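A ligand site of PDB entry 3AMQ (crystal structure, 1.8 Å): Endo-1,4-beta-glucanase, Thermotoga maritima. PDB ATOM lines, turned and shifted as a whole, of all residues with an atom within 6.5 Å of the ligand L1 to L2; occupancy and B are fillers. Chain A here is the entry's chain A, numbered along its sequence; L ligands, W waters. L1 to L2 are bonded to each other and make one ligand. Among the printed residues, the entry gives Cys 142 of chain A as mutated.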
ATOM      1  N   GLU A  30      -2.528   0.234 -39.839  1.00  0.00           N
ATOM      2  CA  GLU A  30      -2.353  -1.092 -39.224  1.00  0.00           C
ATOM      3  C   GLU A  30      -3.722  -1.743 -39.192  1.00  0.00           C
ATOM      4  O   GLU A  30      -4.637  -1.187 -38.576  1.00  0.00           O
ATOM      5  CB  GLU A  30      -1.831  -1.057 -37.767  1.00  0.00           C
ATOM      6  CG  GLU A  30      -1.458  -2.474 -37.350  1.00  0.00           C
ATOM      7  CD  GLU A  30      -1.166  -2.644 -35.833  1.00  0.00           C
ATOM      8  OE1 GLU A  30      -0.614  -1.685 -35.236  1.00  0.00           O
ATOM      9  OE2 GLU A  30      -1.485  -3.720 -35.276  1.00  0.00           O
ATOM     10  N   ASN A  32      -5.272  -3.826 -37.569  1.00  0.00           N
ATOM     11  CA  ASN A  32      -5.003  -4.275 -36.204  1.00  0.00           C
ATOM     12  C   ASN A  32      -6.114  -5.111 -35.595  1.00  0.00           C
ATOM     13  O   ASN A  32      -7.187  -4.589 -35.303  1.00  0.00           O
ATOM     14  CB  ASN A  32      -4.685  -2.980 -35.375  1.00  0.00           C
ATOM     15  CG  ASN A  32      -4.434  -3.269 -33.907  1.00  0.00           C
ATOM     16  OD1 ASN A  32      -4.578  -4.393 -33.440  1.00  0.00           O
ATOM     17  ND2 ASN A  32      -4.077  -2.197 -33.148  1.00  0.00           N
ATOM     18  N   TRP A  34      -5.495  -7.082 -32.891  1.00  0.00           N
ATOM     19  CA  TRP A  34      -4.578  -7.546 -31.827  1.00  0.00           C
ATOM     20  C   TRP A  34      -5.089  -8.549 -30.805  1.00  0.00           C
ATOM     21  O   TRP A  34      -4.311  -9.357 -30.318  1.00  0.00           O
ATOM     22  CB  TRP A  34      -3.947  -6.334 -31.104  1.00  0.00           C
ATOM     23  CG  TRP A  34      -4.924  -5.583 -30.219  1.00  0.00           C
ATOM     24  CD1 TRP A  34      -5.767  -4.546 -30.578  1.00  0.00           C
ATOM     25  CD2 TRP A  34      -5.129  -5.780 -28.793  1.00  0.00           C
ATOM     26  NE1 TRP A  34      -6.454  -4.083 -29.467  1.00  0.00           N
ATOM     27  CE2 TRP A  34      -6.074  -4.821 -28.367  1.00  0.00           C
ATOM     28  CE3 TRP A  34      -4.595  -6.676 -27.860  1.00  0.00           C
ATOM     29  CZ2 TRP A  34      -6.502  -4.722 -27.014  1.00  0.00           C
ATOM     30  CZ3 TRP A  34      -5.017  -6.581 -26.501  1.00  0.00           C
ATOM     31  CH2 TRP A  34      -5.964  -5.598 -26.103  1.00  0.00           C
ATOM     32  N   GLU A  65      -7.045 -12.852 -25.242  1.00  0.00           N
ATOM     33  CA  GLU A  65      -7.189 -12.618 -23.820  1.00  0.00           C
ATOM     34  C   GLU A  65      -8.566 -11.999 -23.571  1.00  0.00           C
ATOM     35  O   GLU A  65      -8.744 -10.782 -23.784  1.00  0.00           O
ATOM     36  CB  GLU A  65      -6.177 -11.586 -23.265  1.00  0.00           C
ATOM     37  CG  GLU A  65      -4.685 -11.775 -23.507  1.00  0.00           C
ATOM     38  CD  GLU A  65      -3.837 -10.594 -22.947  1.00  0.00           C
ATOM     39  OE1 GLU A  65      -3.506  -9.594 -23.697  1.00  0.00           O
ATOM     40  OE2 GLU A  65      -3.513 -10.649 -21.721  1.00  0.00           O
ATOM     41  N   ARG A  68      -9.090  -8.506 -21.803  1.00  0.00           N
ATOM     42  CA  ARG A  68      -8.846  -7.202 -22.479  1.00  0.00           C
ATOM     43  C   ARG A  68     -10.125  -6.588 -23.079  1.00  0.00           C
ATOM     44  O   ARG A  68     -10.175  -5.402 -23.477  1.00  0.00           O
ATOM     45  CB  ARG A  68      -7.764  -7.352 -23.560  1.00  0.00           C
ATOM     46  CG  ARG A  68      -6.474  -7.927 -23.052  1.00  0.00           C
ATOM     47  CD  ARG A  68      -5.931  -7.162 -21.813  1.00  0.00           C
ATOM     48  NE  ARG A  68      -5.795  -5.738 -22.120  1.00  0.00           N
ATOM     49  CZ  ARG A  68      -4.807  -5.233 -22.860  1.00  0.00           C
ATOM     50  NH1 ARG A  68      -3.857  -6.027 -23.354  1.00  0.00           N
ATOM     51  NH2 ARG A  68      -4.762  -3.938 -23.099  1.00  0.00           N
ATOM     52  N   VAL A  70     -12.003  -5.704 -25.659  1.00  0.00           N
ATOM     53  CA  VAL A  70     -12.194  -5.505 -27.118  1.00  0.00           C
ATOM     54  C   VAL A  70     -11.410  -6.558 -27.932  1.00  0.00           C
ATOM     55  O   VAL A  70     -10.565  -7.300 -27.378  1.00  0.00           O
ATOM     56  CB  VAL A  70     -11.784  -4.029 -27.589  1.00  0.00           C
ATOM     57  CG1 VAL A  70     -12.613  -2.996 -26.851  1.00  0.00           C
ATOM     58  CG2 VAL A  70     -10.323  -3.809 -27.385  1.00  0.00           C
ATOM     59  N   GLY A  72     -10.181  -5.737 -31.474  1.00  0.00           N
ATOM     60  CA  GLY A  72      -9.174  -5.127 -32.348  1.00  0.00           C
ATOM     61  C   GLY A  72      -9.319  -3.626 -32.417  1.00  0.00           C
ATOM     62  O   GLY A  72     -10.216  -3.033 -31.794  1.00  0.00           O
ATOM     63  N   TYR A  73      -8.403  -3.000 -33.165  1.00  0.00           N
ATOM     64  CA  TYR A  73      -8.392  -1.547 -33.350  1.00  0.00           C
ATOM     65  C   TYR A  73      -7.812  -1.133 -34.726  1.00  0.00           C
ATOM     66  O   TYR A  73      -6.728  -0.567 -34.826  1.00  0.00           O
ATOM     67  CB  TYR A  73      -7.602  -0.952 -32.178  1.00  0.00           C
ATOM     68  CG  TYR A  73      -7.441   0.573 -32.159  1.00  0.00           C
ATOM     69  CD1 TYR A  73      -8.526   1.422 -32.166  1.00  0.00           C
ATOM     70  CD2 TYR A  73      -6.155   1.127 -32.066  1.00  0.00           C
ATOM     71  CE1 TYR A  73      -8.370   2.819 -32.070  1.00  0.00           C
ATOM     72  CE2 TYR A  73      -5.964   2.500 -31.973  1.00  0.00           C
ATOM     73  CZ  TYR A  73      -7.077   3.332 -31.978  1.00  0.00           C
ATOM     74  OH  TYR A  73      -6.850   4.682 -31.859  1.00  0.00           O
ATOM     75  N   GLU A  75      -6.645   0.874 -37.630  1.00  0.00           N
ATOM     76  CA  GLU A  75      -6.245   2.253 -37.429  1.00  0.00           C
ATOM     77  C   GLU A  75      -5.107   2.711 -38.385  1.00  0.00           C
ATOM     78  O   GLU A  75      -4.485   1.903 -39.122  1.00  0.00           O
ATOM     79  CB  GLU A  75      -5.627   2.307 -36.007  1.00  0.00           C
ATOM     80  CG  GLU A  75      -4.283   1.440 -35.924  1.00  0.00           C
ATOM     81  CD  GLU A  75      -3.567   1.521 -34.592  1.00  0.00           C
ATOM     82  OE1 GLU A  75      -3.064   2.630 -34.203  1.00  0.00           O
ATOM     83  OE2 GLU A  75      -3.462   0.499 -33.905  1.00  0.00           O
ATOM     84  N   LYS A  81       4.717   3.740 -32.841  1.00  0.00           N
ATOM     85  CA  LYS A  81       3.775   2.965 -31.994  1.00  0.00           C
ATOM     86  C   LYS A  81       4.683   2.003 -31.213  1.00  0.00           C
ATOM     87  O   LYS A  81       5.266   1.082 -31.772  1.00  0.00           O
ATOM     88  CB  LYS A  81       2.774   2.183 -32.872  1.00  0.00           C
ATOM     89  CG  LYS A  81       1.927   1.234 -32.041  1.00  0.00           C
ATOM     90  CD  LYS A  81       0.759   0.713 -32.841  1.00  0.00           C
ATOM     91  CE  LYS A  81      -0.126  -0.112 -31.914  1.00  0.00           C
ATOM     92  NZ  LYS A  81      -1.199  -0.889 -32.660  1.00  0.00           N
ATOM     93  N   TRP A  83       4.158  -0.588 -29.227  1.00  0.00           N
ATOM     94  CA  TRP A  83       3.889  -2.004 -29.288  1.00  0.00           C
ATOM     95  C   TRP A  83       4.406  -2.667 -30.484  1.00  0.00           C
ATOM     96  O   TRP A  83       4.754  -3.835 -30.416  1.00  0.00           O
ATOM     97  CB  TRP A  83       2.404  -2.270 -29.138  1.00  0.00           C
ATOM     98  CG  TRP A  83       1.905  -1.702 -27.866  1.00  0.00           C
ATOM     99  CD1 TRP A  83       1.254  -0.526 -27.689  1.00  0.00           C
ATOM    100  CD2 TRP A  83       2.018  -2.300 -26.564  1.00  0.00           C
ATOM    101  NE1 TRP A  83       0.951  -0.344 -26.343  1.00  0.00           N
ATOM    102  CE2 TRP A  83       1.411  -1.425 -25.636  1.00  0.00           C
ATOM    103  CE3 TRP A  83       2.569  -3.499 -26.105  1.00  0.00           C
ATOM    104  CZ2 TRP A  83       1.344  -1.705 -24.254  1.00  0.00           C
ATOM    105  CZ3 TRP A  83       2.496  -3.799 -24.716  1.00  0.00           C
ATOM    106  CH2 TRP A  83       1.876  -2.892 -23.815  1.00  0.00           C
ATOM    107  N   GLU A  84       4.459  -1.971 -31.611  1.00  0.00           N
ATOM    108  CA  GLU A  84       4.924  -2.636 -32.803  1.00  0.00           C
ATOM    109  C   GLU A  84       6.328  -2.211 -33.202  1.00  0.00           C
ATOM    110  O   GLU A  84       6.742  -2.428 -34.343  1.00  0.00           O
ATOM    111  CB  GLU A  84       3.941  -2.335 -33.951  1.00  0.00           C
ATOM    112  CG  GLU A  84       2.554  -3.030 -33.749  1.00  0.00           C
ATOM    113  CD  GLU A  84       2.697  -4.537 -33.892  1.00  0.00           C
ATOM    114  OE1 GLU A  84       3.583  -4.956 -34.668  1.00  0.00           O
ATOM    115  OE2 GLU A  84       1.962  -5.301 -33.249  1.00  0.00           O
ATOM    116  N   GLU A 124      -5.739   7.934 -30.017  1.00  0.00           N
ATOM    117  CA  GLU A 124      -4.951   7.731 -28.807  1.00  0.00           C
ATOM    118  C   GLU A 124      -3.440   7.921 -28.939  1.00  0.00           C
ATOM    119  O   GLU A 124      -2.872   7.975 -30.042  1.00  0.00           O
ATOM    120  CB  GLU A 124      -5.256   6.357 -28.206  1.00  0.00           C
ATOM    121  CG  GLU A 124      -4.530   5.227 -28.861  1.00  0.00           C
ATOM    122  CD  GLU A 124      -4.604   3.895 -28.061  1.00  0.00           C
ATOM    123  OE1 GLU A 124      -3.971   2.956 -28.468  1.00  0.00           O
ATOM    124  OE2 GLU A 124      -5.297   3.766 -27.022  1.00  0.00           O
ATOM    125  N   TRP A 126       0.480   7.101 -26.618  1.00  0.00           N
ATOM    126  CA  TRP A 126       1.140   6.377 -25.577  1.00  0.00           C
ATOM    127  C   TRP A 126       2.262   7.285 -25.052  1.00  0.00           C
ATOM    128  O   TRP A 126       3.159   7.621 -25.810  1.00  0.00           O
ATOM    129  CB  TRP A 126       1.776   5.105 -26.116  1.00  0.00           C
ATOM    130  CG  TRP A 126       0.749   4.123 -26.535  1.00  0.00           C
ATOM    131  CD1 TRP A 126       0.172   4.035 -27.777  1.00  0.00           C
ATOM    132  CD2 TRP A 126       0.081   3.124 -25.708  1.00  0.00           C
ATOM    133  NE1 TRP A 126      -0.795   3.060 -27.767  1.00  0.00           N
ATOM    134  CE2 TRP A 126      -0.872   2.493 -26.524  1.00  0.00           C
ATOM    135  CE3 TRP A 126       0.217   2.718 -24.355  1.00  0.00           C
ATOM    136  CZ2 TRP A 126      -1.704   1.464 -26.042  1.00  0.00           C
ATOM    137  CZ3 TRP A 126      -0.622   1.692 -23.865  1.00  0.00           C
ATOM    138  CH2 TRP A 126      -1.565   1.078 -24.709  1.00  0.00           C
ATOM    139  N   CYS A 142      -1.667   5.803 -21.376  1.00  0.00           N
ATOM    140  CA  CYS A 142      -2.356   5.693 -22.646  1.00  0.00           C
ATOM    141  C   CYS A 142      -3.448   6.756 -22.529  1.00  0.00           C
ATOM    142  O   CYS A 142      -4.186   6.766 -21.527  1.00  0.00           O
ATOM    143  CB  CYS A 142      -3.077   4.353 -22.792  1.00  0.00           C
ATOM    144  SG  CYS A 142      -4.026   4.341 -24.328  1.00  0.00           S
ATOM    145  N   MET A 144      -6.777   8.294 -24.528  1.00  0.00           N
ATOM    146  CA  MET A 144      -7.648   8.106 -25.689  1.00  0.00           C
ATOM    147  C   MET A 144      -8.642   9.243 -25.740  1.00  0.00           C
ATOM    148  O   MET A 144      -8.993   9.838 -24.683  1.00  0.00           O
ATOM    149  CB  MET A 144      -8.456   6.797 -25.539  1.00  0.00           C
ATOM    150  CG  MET A 144      -7.577   5.537 -25.320  1.00  0.00           C
ATOM    151  SD  MET A 144      -8.623   4.017 -25.526  1.00  0.00           S
ATOM    152  CE  MET A 144      -8.591   3.981 -27.385  1.00  0.00           C
ATOM    153  N   TRP A 184      -4.123   0.033 -14.635  1.00  0.00           N
ATOM    154  CA  TRP A 184      -3.868  -1.350 -15.004  1.00  0.00           C
ATOM    155  C   TRP A 184      -2.361  -1.542 -15.007  1.00  0.00           C
ATOM    156  O   TRP A 184      -1.685  -1.118 -14.057  1.00  0.00           O
ATOM    157  CB  TRP A 184      -4.422  -1.651 -16.399  1.00  0.00           C
ATOM    158  CG  TRP A 184      -5.913  -1.558 -16.547  1.00  0.00           C
ATOM    159  CD1 TRP A 184      -6.875  -1.955 -15.630  1.00  0.00           C
ATOM    160  CD2 TRP A 184      -6.628  -1.139 -17.723  1.00  0.00           C
ATOM    161  NE1 TRP A 184      -8.142  -1.808 -16.167  1.00  0.00           N
ATOM    162  CE2 TRP A 184      -8.020  -1.308 -17.450  1.00  0.00           C
ATOM    163  CE3 TRP A 184      -6.232  -0.632 -18.973  1.00  0.00           C
ATOM    164  CZ2 TRP A 184      -9.003  -0.991 -18.391  1.00  0.00           C
ATOM    165  CZ3 TRP A 184      -7.220  -0.323 -19.914  1.00  0.00           C
ATOM    166  CH2 TRP A 184      -8.587  -0.508 -19.614  1.00  0.00           C
ATOM    167  N   TRP A 186      -0.532  -0.043 -16.861  1.00  0.00           N
ATOM    168  CA  TRP A 186      -0.044   1.300 -17.126  1.00  0.00           C
ATOM    169  C   TRP A 186      -1.277   2.076 -16.841  1.00  0.00           C
ATOM    170  O   TRP A 186      -2.327   1.492 -16.573  1.00  0.00           O
ATOM    171  CB  TRP A 186       0.408   1.460 -18.597  1.00  0.00           C
ATOM    172  CG  TRP A 186      -0.623   0.986 -19.603  1.00  0.00           C
ATOM    173  CD1 TRP A 186      -1.708   1.665 -20.045  1.00  0.00           C
ATOM    174  CD2 TRP A 186      -0.669  -0.308 -20.236  1.00  0.00           C
ATOM    175  NE1 TRP A 186      -2.447   0.875 -20.904  1.00  0.00           N
ATOM    176  CE2 TRP A 186      -1.833  -0.347 -21.030  1.00  0.00           C
ATOM    177  CE3 TRP A 186       0.157  -1.439 -20.189  1.00  0.00           C
ATOM    178  CZ2 TRP A 186      -2.195  -1.476 -21.789  1.00  0.00           C
ATOM    179  CZ3 TRP A 186      -0.182  -2.560 -20.935  1.00  0.00           C
ATOM    180  CH2 TRP A 186      -1.370  -2.558 -21.742  1.00  0.00           C
ATOM    181  N   TYR A 188      -4.470   4.189 -17.863  1.00  0.00           N
ATOM    182  CA  TYR A 188      -5.318   4.361 -19.020  1.00  0.00           C
ATOM    183  C   TYR A 188      -6.262   5.522 -18.712  1.00  0.00           C
ATOM    184  O   TYR A 188      -6.952   5.499 -17.700  1.00  0.00           O
ATOM    185  CB  TYR A 188      -6.119   3.049 -19.238  1.00  0.00           C
ATOM    186  CG  TYR A 188      -7.349   3.137 -20.119  1.00  0.00           C
ATOM    187  CD1 TYR A 188      -7.308   2.722 -21.466  1.00  0.00           C
ATOM    188  CD2 TYR A 188      -8.579   3.543 -19.598  1.00  0.00           C
ATOM    189  CE1 TYR A 188      -8.449   2.716 -22.261  1.00  0.00           C
ATOM    190  CE2 TYR A 188      -9.761   3.516 -20.398  1.00  0.00           C
ATOM    191  CZ  TYR A 188      -9.667   3.101 -21.721  1.00  0.00           C
ATOM    192  OH  TYR A 188     -10.800   3.030 -22.489  1.00  0.00           O
ATOM    193  N   GLU A 235      -2.652   7.870 -32.827  1.00  0.00           N
ATOM    194  CA  GLU A 235      -3.427   6.819 -33.497  1.00  0.00           C
ATOM    195  C   GLU A 235      -4.873   7.232 -33.672  1.00  0.00           C
ATOM    196  O   GLU A 235      -5.457   7.846 -32.820  1.00  0.00           O
ATOM    197  CB  GLU A 235      -3.397   5.500 -32.696  1.00  0.00           C
ATOM    198  CG  GLU A 235      -1.943   5.025 -32.416  1.00  0.00           C
ATOM    199  CD  GLU A 235      -1.886   3.812 -31.530  1.00  0.00           C
ATOM    200  OE1 GLU A 235      -1.573   4.031 -30.320  1.00  0.00           O
ATOM    201  OE2 GLU A 235      -2.162   2.667 -32.004  1.00  0.00           O
ATOM    202  N   GLU A 239     -11.988   0.892 -32.075  1.00  0.00           N
ATOM    203  CA  GLU A 239     -11.921  -0.368 -31.318  1.00  0.00           C
ATOM    204  C   GLU A 239     -13.281  -1.081 -31.515  1.00  0.00           C
ATOM    205  O   GLU A 239     -14.317  -0.428 -31.733  1.00  0.00           O
ATOM    206  CB  GLU A 239     -11.788  -0.103 -29.807  1.00  0.00           C
ATOM    207  CG  GLU A 239     -10.556   0.617 -29.425  1.00  0.00           C
ATOM    208  CD  GLU A 239     -10.386   0.567 -27.884  1.00  0.00           C
ATOM    209  OE1 GLU A 239      -9.778  -0.403 -27.383  1.00  0.00           O
ATOM    210  OE2 GLU A 239     -10.922   1.459 -27.222  1.00  0.00           O
HETATM  211  C1  LIG L   1      -6.845   0.537 -25.203  1.00  0.00           C
HETATM  212  C2  LIG L   1      -6.050  -0.644 -24.645  1.00  0.00           C
HETATM  213  C3  LIG L   1      -4.778  -0.856 -25.463  1.00  0.00           C
HETATM  214  C4  LIG L   1      -5.118  -1.063 -26.940  1.00  0.00           C
HETATM  215  C5  LIG L   1      -6.034   0.057 -27.420  1.00  0.00           C
HETATM  216  C6  LIG L   1      -6.585  -0.331 -28.795  1.00  0.00           C
HETATM  217  O1  LIG L   1      -6.049   1.728 -25.114  1.00  0.00           O
HETATM  218  O2  LIG L   1      -5.690  -0.344 -23.295  1.00  0.00           O
HETATM  219  O3  LIG L   1      -4.097  -1.996 -24.954  1.00  0.00           O
HETATM  220  O4  LIG L   1      -3.930  -1.024 -27.748  1.00  0.00           O
HETATM  221  O5  LIG L   1      -7.179   0.279 -26.582  1.00  0.00           O
HETATM  222  O6  LIG L   1      -7.488  -1.418 -28.614  1.00  0.00           O
HETATM  223  C1  LG2 L   2      -2.474  -2.096 -29.312  1.00  0.00           C
HETATM  224  C2  LG2 L   2      -1.824  -3.410 -29.739  1.00  0.00           C
HETATM  225  C3  LG2 L   2      -1.020  -3.938 -28.549  1.00  0.00           C
HETATM  226  C4  LG2 L   2      -1.880  -4.008 -27.286  1.00  0.00           C
HETATM  227  C5  LG2 L   2      -0.980  -4.396 -26.114  1.00  0.00           C
HETATM  228  C6  LG2 L   2      -3.356  -2.296 -28.078  1.00  0.00           C
HETATM  229  O1  LG2 L   2      -3.266  -1.549 -30.382  1.00  0.00           O
HETATM  230  O2  LG2 L   2      -0.953  -3.175 -30.852  1.00  0.00           O
HETATM  231  O3  LG2 L   2      -0.558  -5.266 -28.823  1.00  0.00           O
HETATM  232  O4  LG2 L   2      -2.542  -2.761 -26.994  1.00  0.00           O
HETATM  233  O5  LG2 L   2      -1.786  -4.517 -24.933  1.00  0.00           O
HETATM  234  C1  LG3 L   3     -12.312  -0.185 -23.222  1.00  0.00           C
HETATM  235  C2  LG3 L   3     -11.271  -0.151 -24.362  1.00  0.00           C
HETATM  236  C3  LG3 L   3      -9.991  -0.892 -23.976  1.00  0.00           C
HETATM  237  C4  LG3 L   3     -10.223  -2.214 -23.202  1.00  0.00           C
HETATM  238  C5  LG3 L   3      -8.923  -2.819 -22.631  1.00  0.00           C
HETATM  239  C6  LG3 L   3     -12.398  -1.572 -22.550  1.00  0.00           C
HETATM  240  O1  LG3 L   3     -13.259  -1.525 -21.469  1.00  0.00           O
HETATM  241  O2  LG3 L   3     -13.592   0.154 -23.734  1.00  0.00           O
HETATM  242  O3  LG3 L   3     -10.926   1.203 -24.682  1.00  0.00           O
HETATM  243  O4  LG3 L   3      -9.284  -1.177 -25.164  1.00  0.00           O
HETATM  244  O5  LG3 L   3     -11.114  -1.976 -22.095  1.00  0.00           O
HETATM  245  O6  LG3 L   3      -8.080  -3.349 -23.661  1.00  0.00           O
HETATM  246  O   HOH W   1      -0.768  -4.703 -32.989  1.00  0.00           O
HETATM  247  O   HOH W   2       1.710  -5.666 -30.271  1.00  0.00           O
HETATM  248  O   HOH W   3      -2.905   1.049 -30.013  1.00  0.00           O
HETATM  249  O   HOH W   4      -0.798  -7.727 -27.838  1.00  0.00           O
HETATM  250  O   HOH W   5      -0.531  -5.809 -22.725  1.00  0.00           O
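The guanidinium group of Arg 68 lies within hydrogen-bond range of an oxygen (O3) of LIG L1 (2.8 Å).
OE1 of Glu 239 sits at hydrogen-bond distance from O6 of LIG L1.
The side-chain carboxylate of Glu 124 is in hydrogen-bond range of an oxygen (O1) of LIG L1 (2.9 Å).
NZ of Lys 81 is in hydrogen-bond range of O2 of LG2 L2, at 2.9 Å.
O1 of LG2 L2 is in hydrogen-bond range of ND2 of Asn 32, at 3.0 Å.
NE1 of Trp 34 lies within hydrogen-bond range of O6 of LIG L1, at 3.0 Å.
An oxygen (O1) of LIG L1 is in hydrogen-bond range of the side-chain sulfur of Cys 142 (3.4 Å).
The side-chain sulfur of Met 144 is in hydrogen-bond range of an oxygen (O1) of LIG L1 (3.5 Å).
The backbone carbonyl oxygen of Arg 68 sits at hydrogen-bond distance from an oxygen (O6) of LG3 L3.
An oxygen (O6) of LG3 L3 is in hydrogen-bond range of the guanidinium group of Arg 68 (3.4 Å).
The side-chain carboxylate of Glu 239 lies within hydrogen-bond range of an oxygen (O4) of LG3 L3 (2.4 Å).
The side-chain sulfur (SD) of Met 144 is in hydrogen-bond range of an oxygen (O3) of LG3 L3, at 3.7 Å.
OH of Tyr 188 is in hydrogen-bond range of O3 of LG3 L3 (2.9 Å).
Water W1 lies within hydrogen-bond range of the side-chain carboxylate of Glu 30 (2.6 Å), an oxygen (O2) of LG2 L2 (2.6 Å) and the side-chain carboxylate of Glu 84 (2.8 Å).
Water W3 lies within hydrogen-bond range of O1 of LG2 L2 (2.6 Å), OE2 of Glu 235 (2.7 Å) and OE1 of Glu 124 (2.7 Å).
Water W2 bridges O3 of LG2 L2 (2.7 Å) and OE2 of Glu 84 (3.0 Å).
Water W5 bridges an oxygen (O5) of LG2 L2 (2.8 Å) and the guanidinium group of Arg 68 (3.4 Å).
An oxygen (O5) of LIG L1 is in hydrogen-bond range of an oxygen (O4) of LG3 L3 (2.9 Å).
The guanidinium group of Arg 68 is in salt-bridge range of the side-chain carboxylate of Glu 65 (3.6 Å).
The side-chain carboxylate (OE1) of Glu 124 sits at hydrogen-bond distance from the indole nitrogen (NE1) of Trp 126, at 3.3 Å.
The backbone carbonyl oxygen (O) of Glu 124 is in hydrogen-bond range of the backbone NH (N) of Glu 235 (2.8 Å).
The side-chain amino group (NZ) of Lys 81 lies close to the side-chain amide nitrogen (ND2) of Asn 32.
OE1 of Glu 30 lies within salt-bridge range of NZ of Lys 81 (2.8 Å).
The backbone carbonyl oxygen of Asn 32 is in hydrogen-bond range of the backbone NH of Tyr 73 (2.9 Å).
ND2 of Asn 32 sits at hydrogen-bond distance from OE2 of Glu 75, 2.9 Å away.
The indole nitrogen (NE1) of Trp 126 sits at hydrogen-bond distance from the side-chain carboxylate (OE1) of Glu 235.
Merely in contact with the ligand L1 to L2: Tyr 73, Trp 83, Trp 184, Trp 186, Trp 126, Tyr 188 and Val 70.
Hydrophobic or aromatic side chains that line the ligand L1 to L2: Trp 34, Val 70, Tyr 73, Trp 83, Trp 126, Met 144, Trp 184, Trp 186 and Tyr 188.
The nearest printed residue that does not touch the ligand L1 to L2 is Glu 75 (4.1 Å).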
